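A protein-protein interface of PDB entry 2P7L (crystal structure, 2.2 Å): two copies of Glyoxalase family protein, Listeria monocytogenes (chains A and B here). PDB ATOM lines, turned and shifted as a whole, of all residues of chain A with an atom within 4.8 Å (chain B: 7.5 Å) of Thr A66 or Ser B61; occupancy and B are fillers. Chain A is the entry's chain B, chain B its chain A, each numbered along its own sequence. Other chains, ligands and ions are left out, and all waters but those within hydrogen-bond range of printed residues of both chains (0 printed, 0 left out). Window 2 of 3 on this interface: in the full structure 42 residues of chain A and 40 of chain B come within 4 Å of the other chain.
Printed residues of chain B that touch a printed residue of chain A: Ile B11, Met B57, Ser B61, Gln B63 and His B115.
Hydrophobic or aromatic side chains of chain B within 4 Å of the printed part of chain A: Ile B11, Met B57 and His B115.
Printed residues of chain A that touch a printed residue of chain B: Glu A64, Thr A66, Tyr A67 and Asn A68.
Among the printed residues, 7 pairs touch across the chains.
Among the printed residues, no Asp or Glu carboxylate lies within 4 Å of a Lys or Arg side-chain nitrogen of the other chain.
Of the printed residues of chain B, Glu A64 touches Gln B63 (2.9 Å).
Printed residues of chain B within 4 Å of Thr A66: Ser B61 and Gln B63.
Printed residues of chain B within 4 Å of Asn A68: Ile B11 (2.7 Å) and His B115 (2.8 Å).
Val B12 touches none of the printed residues of chain A.
Of the printed residues of chain A, Met B57 touches Tyr A67.
Ser B61 touches just one residue of chain A: Thr A66.
Of the printed residues of chain A, His B115 touches Asn A68.
The nearest residue of chain A that does not touch Ser B61 is Tyr A67 (4.5 Å).
The nearest printed residue of chain B that does not touch Glu A64 is Glu B64 (4.4 Å).
O of Met B57 lies within hydrogen-bond range of N of Val B12 (2.9 Å).
OE1 of Gln B63 lies close to OE1 of Glu B64 (2.8 Å).
The side-chain hydroxyl (OG1) of Thr A66 sits at hydrogen-bond distance from the side-chain amide nitrogen (ND2) of Asn A68, at 3.1 Å.
N of Ile B11 is in hydrogen-bond range of OD1 of Asn A68 (2.7 Å).
The side-chain amide oxygen (OE1) of Gln B63 sits close to the backbone carbonyl oxygen (O) of Glu A64 (2.9 Å).
The side-chain hydroxyl (OG1) of Thr A66 is in hydrogen-bond range of the side-chain amide nitrogen (NE2) of Gln B63 (2.8 Å).
NE2 of His B115 lies within hydrogen-bond range of OD1 of Asn A68, at 2.8 Å.
Position printed for both chains: 64.
Of the 7 pairs that touch across the chains among the printed residues, none has its exchanged pair printed and touching as well.
Ser B61 touches Thr A66 (OG to CG2, 3.3 Å).
Tyr A67 touches Ile B11 (CB to CD1, 3.8 Å).
Tyr A67 touches Met B57.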
ATOM      1  N   GLU A  64      -6.797  20.663   4.796  1.00  0.00           N
ATOM      2  CA  GLU A  64      -7.476  21.695   4.007  1.00  0.00           C
ATOM      3  C   GLU A  64      -6.822  21.768   2.630  1.00  0.00           C
ATOM      4  O   GLU A  64      -5.660  21.391   2.468  1.00  0.00           O
ATOM      5  CB  GLU A  64      -7.346  23.074   4.667  1.00  0.00           C
ATOM      6  CG  GLU A  64      -7.817  23.150   6.110  1.00  0.00           C
ATOM      7  CD  GLU A  64      -9.313  23.379   6.243  1.00  0.00           C
ATOM      8  OE1 GLU A  64     -10.092  22.723   5.513  1.00  0.00           O
ATOM      9  OE2 GLU A  64      -9.703  24.214   7.089  1.00  0.00           O
ATOM     10  N   ARG A  65      -7.561  22.266   1.645  1.00  0.00           N
ATOM     11  CA  ARG A  65      -7.027  22.402   0.294  1.00  0.00           C
ATOM     12  C   ARG A  65      -6.570  23.839   0.042  1.00  0.00           C
ATOM     13  O   ARG A  65      -7.283  24.784   0.379  1.00  0.00           O
ATOM     14  CB  ARG A  65      -8.087  22.014  -0.739  1.00  0.00           C
ATOM     15  CG  ARG A  65      -8.486  20.540  -0.693  1.00  0.00           C
ATOM     16  CD  ARG A  65      -9.577  20.212  -1.706  1.00  0.00           C
ATOM     17  NE  ARG A  65      -9.819  18.775  -1.781  1.00  0.00           N
ATOM     18  CZ  ARG A  65     -10.688  18.200  -2.610  1.00  0.00           C
ATOM     19  NH1 ARG A  65     -11.410  18.939  -3.441  1.00  0.00           N
ATOM     20  NH2 ARG A  65     -10.818  16.882  -2.618  1.00  0.00           N
ATOM     21  N   THR A  66      -5.374  23.986  -0.533  1.00  0.00           N
ATOM     22  CA  THR A  66      -4.799  25.291  -0.863  1.00  0.00           C
ATOM     23  C   THR A  66      -4.329  25.250  -2.315  1.00  0.00           C
ATOM     24  O   THR A  66      -4.331  24.190  -2.943  1.00  0.00           O
ATOM     25  CB  THR A  66      -3.592  25.646   0.038  1.00  0.00           C
ATOM     26  OG1 THR A  66      -2.568  24.654  -0.110  1.00  0.00           O
ATOM     27  CG2 THR A  66      -4.012  25.715   1.505  1.00  0.00           C
ATOM     28  N   TYR A  67      -3.921  26.396  -2.851  1.00  0.00           N
ATOM     29  CA  TYR A  67      -3.483  26.442  -4.231  1.00  0.00           C
ATOM     30  C   TYR A  67      -2.021  26.059  -4.432  1.00  0.00           C
ATOM     31  O   TYR A  67      -1.532  26.047  -5.555  1.00  0.00           O
ATOM     32  CB  TYR A  67      -3.742  27.818  -4.830  1.00  0.00           C
ATOM     33  CG  TYR A  67      -3.785  27.790  -6.334  1.00  0.00           C
ATOM     34  CD1 TYR A  67      -4.771  27.056  -7.006  1.00  0.00           C
ATOM     35  CD2 TYR A  67      -2.834  28.470  -7.097  1.00  0.00           C
ATOM     36  CE1 TYR A  67      -4.807  27.002  -8.403  1.00  0.00           C
ATOM     37  CE2 TYR A  67      -2.861  28.421  -8.495  1.00  0.00           C
ATOM     38  CZ  TYR A  67      -3.853  27.684  -9.141  1.00  0.00           C
ATOM     39  OH  TYR A  67      -3.891  27.631 -10.520  1.00  0.00           O
ATOM     40  N   ASN A  68      -1.309  25.764  -3.354  1.00  0.00           N
ATOM     41  CA  ASN A  68       0.073  25.328  -3.515  1.00  0.00           C
ATOM     42  C   ASN A  68      -0.023  24.037  -4.315  1.00  0.00           C
ATOM     43  O   ASN A  68      -0.869  23.188  -4.024  1.00  0.00           O
ATOM     44  CB  ASN A  68       0.714  25.019  -2.165  1.00  0.00           C
ATOM     45  CG  ASN A  68       0.890  26.251  -1.314  1.00  0.00           C
ATOM     46  OD1 ASN A  68       1.831  27.027  -1.507  1.00  0.00           O
ATOM     47  ND2 ASN A  68      -0.025  26.451  -0.374  1.00  0.00           N
ATOM     48  N   LEU A 116      -3.086  19.112  -4.457  1.00  0.00           N
ATOM     49  CA  LEU A 116      -3.554  19.591  -5.744  1.00  0.00           C
ATOM     50  C   LEU A 116      -2.485  19.369  -6.799  1.00  0.00           C
ATOM     51  O   LEU A 116      -1.360  19.837  -6.667  1.00  0.00           O
ATOM     52  CB  LEU A 116      -3.898  21.075  -5.661  1.00  0.00           C
ATOM     53  CG  LEU A 116      -4.295  21.746  -6.978  1.00  0.00           C
ATOM     54  CD1 LEU A 116      -5.550  21.107  -7.556  1.00  0.00           C
ATOM     55  CD2 LEU A 116      -4.524  23.226  -6.719  1.00  0.00           C
ATOM     56  N   ILE B  11       2.153  29.515  -2.483  1.00  0.00           N
ATOM     57  CA  ILE B  11       1.345  30.673  -2.135  1.00  0.00           C
ATOM     58  C   ILE B  11       1.945  31.313  -0.888  1.00  0.00           C
ATOM     59  O   ILE B  11       2.226  30.633   0.088  1.00  0.00           O
ATOM     60  CB  ILE B  11      -0.134  30.282  -1.861  1.00  0.00           C
ATOM     61  CG1 ILE B  11      -0.684  29.426  -3.012  1.00  0.00           C
ATOM     62  CG2 ILE B  11      -0.995  31.545  -1.711  1.00  0.00           C
ATOM     63  CD1 ILE B  11      -0.721  30.115  -4.359  1.00  0.00           C
ATOM     64  N   VAL B  12       2.171  32.620  -0.939  1.00  0.00           N
ATOM     65  CA  VAL B  12       2.755  33.346   0.188  1.00  0.00           C
ATOM     66  C   VAL B  12       2.007  34.658   0.430  1.00  0.00           C
ATOM     67  O   VAL B  12       1.478  35.265  -0.503  1.00  0.00           O
ATOM     68  CB  VAL B  12       4.237  33.671  -0.078  1.00  0.00           C
ATOM     69  CG1 VAL B  12       5.020  32.382  -0.316  1.00  0.00           C
ATOM     70  CG2 VAL B  12       4.354  34.588  -1.291  1.00  0.00           C
ATOM     71  N   LYS B  13       1.966  35.091   1.683  1.00  0.00           N
ATOM     72  CA  LYS B  13       1.282  36.333   2.021  1.00  0.00           C
ATOM     73  C   LYS B  13       2.049  37.571   1.556  1.00  0.00           C
ATOM     74  O   LYS B  13       1.450  38.524   1.068  1.00  0.00           O
ATOM     75  CB  LYS B  13       1.030  36.413   3.525  1.00  0.00           C
ATOM     76  CG  LYS B  13       2.258  36.229   4.379  1.00  0.00           C
ATOM     77  CD  LYS B  13       1.931  36.488   5.842  1.00  0.00           C
ATOM     78  CE  LYS B  13       3.074  36.064   6.748  1.00  0.00           C
ATOM     79  NZ  LYS B  13       3.308  34.592   6.644  1.00  0.00           N
ATOM     80  N   MET B  57       2.971  32.984  -5.864  1.00  0.00           N
ATOM     81  CA  MET B  57       1.773  33.811  -5.968  1.00  0.00           C
ATOM     82  C   MET B  57       1.394  34.394  -4.604  1.00  0.00           C
ATOM     83  O   MET B  57       1.486  33.714  -3.575  1.00  0.00           O
ATOM     84  CB  MET B  57       0.594  32.989  -6.490  1.00  0.00           C
ATOM     85  CG  MET B  57       0.709  32.488  -7.925  1.00  0.00           C
ATOM     86  SD  MET B  57      -0.747  31.441  -8.384  1.00  0.00           S
ATOM     87  CE  MET B  57      -2.055  32.660  -8.346  1.00  0.00           C
ATOM     88  N   GLU B  58       0.964  35.655  -4.588  1.00  0.00           N
ATOM     89  CA  GLU B  58       0.570  36.274  -3.326  1.00  0.00           C
ATOM     90  C   GLU B  58      -0.882  35.918  -3.038  1.00  0.00           C
ATOM     91  O   GLU B  58      -1.753  36.092  -3.887  1.00  0.00           O
ATOM     92  CB  GLU B  58       0.753  37.796  -3.384  1.00  0.00           C
ATOM     93  CG  GLU B  58       0.677  38.483  -2.017  1.00  0.00           C
ATOM     94  CD  GLU B  58       1.258  39.902  -2.024  1.00  0.00           C
ATOM     95  OE1 GLU B  58       0.644  40.806  -2.635  1.00  0.00           O
ATOM     96  OE2 GLU B  58       2.339  40.102  -1.417  1.00  0.00           O
ATOM     97  N   GLY B  59      -1.122  35.395  -1.841  1.00  0.00           N
ATOM     98  CA  GLY B  59      -2.457  34.999  -1.429  1.00  0.00           C
ATOM     99  C   GLY B  59      -2.472  34.811   0.075  1.00  0.00           C
ATOM    100  O   GLY B  59      -1.413  34.643   0.685  1.00  0.00           O
ATOM    101  N   ASP B  60      -3.657  34.828   0.682  1.00  0.00           N
ATOM    102  CA  ASP B  60      -3.759  34.688   2.132  1.00  0.00           C
ATOM    103  C   ASP B  60      -3.902  33.237   2.572  1.00  0.00           C
ATOM    104  O   ASP B  60      -4.056  32.948   3.762  1.00  0.00           O
ATOM    105  CB  ASP B  60      -4.929  35.534   2.666  1.00  0.00           C
ATOM    106  CG  ASP B  60      -6.173  34.705   2.989  1.00  0.00           C
ATOM    107  OD1 ASP B  60      -6.679  33.991   2.093  1.00  0.00           O
ATOM    108  OD2 ASP B  60      -6.651  34.779   4.148  1.00  0.00           O
ATOM    109  N   SER B  61      -3.837  32.325   1.606  1.00  0.00           N
ATOM    110  CA  SER B  61      -3.957  30.897   1.881  1.00  0.00           C
ATOM    111  C   SER B  61      -2.716  30.425   2.641  1.00  0.00           C
ATOM    112  O   SER B  61      -1.599  30.854   2.342  1.00  0.00           O
ATOM    113  CB  SER B  61      -4.098  30.133   0.562  1.00  0.00           C
ATOM    114  OG  SER B  61      -4.748  28.888   0.746  1.00  0.00           O
ATOM    115  N   LEU B  62      -2.915  29.549   3.625  1.00  0.00           N
ATOM    116  CA  LEU B  62      -1.818  29.024   4.437  1.00  0.00           C
ATOM    117  C   LEU B  62      -2.043  27.568   4.845  1.00  0.00           C
ATOM    118  O   LEU B  62      -2.954  27.259   5.617  1.00  0.00           O
ATOM    119  CB  LEU B  62      -1.647  29.867   5.698  1.00  0.00           C
ATOM    120  CG  LEU B  62      -0.631  29.344   6.711  1.00  0.00           C
ATOM    121  CD1 LEU B  62       0.758  29.347   6.093  1.00  0.00           C
ATOM    122  CD2 LEU B  62      -0.659  30.219   7.952  1.00  0.00           C
ATOM    123  N   GLN B  63      -1.194  26.679   4.337  1.00  0.00           N
ATOM    124  CA  GLN B  63      -1.293  25.256   4.643  1.00  0.00           C
ATOM    125  C   GLN B  63      -0.693  24.987   6.019  1.00  0.00           C
ATOM    126  O   GLN B  63       0.324  25.581   6.381  1.00  0.00           O
ATOM    127  CB  GLN B  63      -0.530  24.451   3.587  1.00  0.00           C
ATOM    128  CG  GLN B  63      -0.830  22.954   3.569  1.00  0.00           C
ATOM    129  CD  GLN B  63      -2.172  22.635   2.924  1.00  0.00           C
ATOM    130  OE1 GLN B  63      -3.203  22.555   3.598  1.00  0.00           O
ATOM    131  NE2 GLN B  63      -2.164  22.464   1.608  1.00  0.00           N
ATOM    132  N   GLU B  64      -1.317  24.105   6.795  1.00  0.00           N
ATOM    133  CA  GLU B  64      -0.778  23.779   8.111  1.00  0.00           C
ATOM    134  C   GLU B  64       0.574  23.115   7.857  1.00  0.00           C
ATOM    135  O   GLU B  64       0.776  22.499   6.804  1.00  0.00           O
ATOM    136  CB  GLU B  64      -1.697  22.800   8.864  1.00  0.00           C
ATOM    137  CG  GLU B  64      -1.641  21.351   8.372  1.00  0.00           C
ATOM    138  CD  GLU B  64      -2.542  21.073   7.170  1.00  0.00           C
ATOM    139  OE1 GLU B  64      -2.744  21.972   6.328  1.00  0.00           O
ATOM    140  OE2 GLU B  64      -3.038  19.932   7.056  1.00  0.00           O
ATOM    141  N   ASP B 113       5.904  31.062   5.072  1.00  0.00           N
ATOM    142  CA  ASP B 113       4.534  30.608   4.908  1.00  0.00           C
ATOM    143  C   ASP B 113       4.326  29.102   5.055  1.00  0.00           C
ATOM    144  O   ASP B 113       3.604  28.478   4.279  1.00  0.00           O
ATOM    145  CB  ASP B 113       4.038  31.099   3.547  1.00  0.00           C
ATOM    146  CG  ASP B 113       4.035  32.630   3.447  1.00  0.00           C
ATOM    147  OD1 ASP B 113       3.007  33.251   3.795  1.00  0.00           O
ATOM    148  OD2 ASP B 113       5.068  33.207   3.038  1.00  0.00           O
ATOM    149  N   HIS B 115       6.242  26.659   4.400  1.00  0.00           N
ATOM    150  CA  HIS B 115       6.813  25.776   3.385  1.00  0.00           C
ATOM    151  C   HIS B 115       8.122  25.174   3.877  1.00  0.00           C
ATOM    152  O   HIS B 115       9.099  25.886   4.114  1.00  0.00           O
ATOM    153  CB  HIS B 115       7.065  26.525   2.084  1.00  0.00           C
ATOM    154  CG  HIS B 115       5.816  26.942   1.385  1.00  0.00           C
ATOM    155  ND1 HIS B 115       5.469  28.264   1.210  1.00  0.00           N
ATOM    156  CD2 HIS B 115       4.824  26.213   0.822  1.00  0.00           C
ATOM    157  CE1 HIS B 115       4.316  28.333   0.566  1.00  0.00           C
ATOM    158  NE2 HIS B 115       3.903  27.101   0.319  1.00  0.00           N
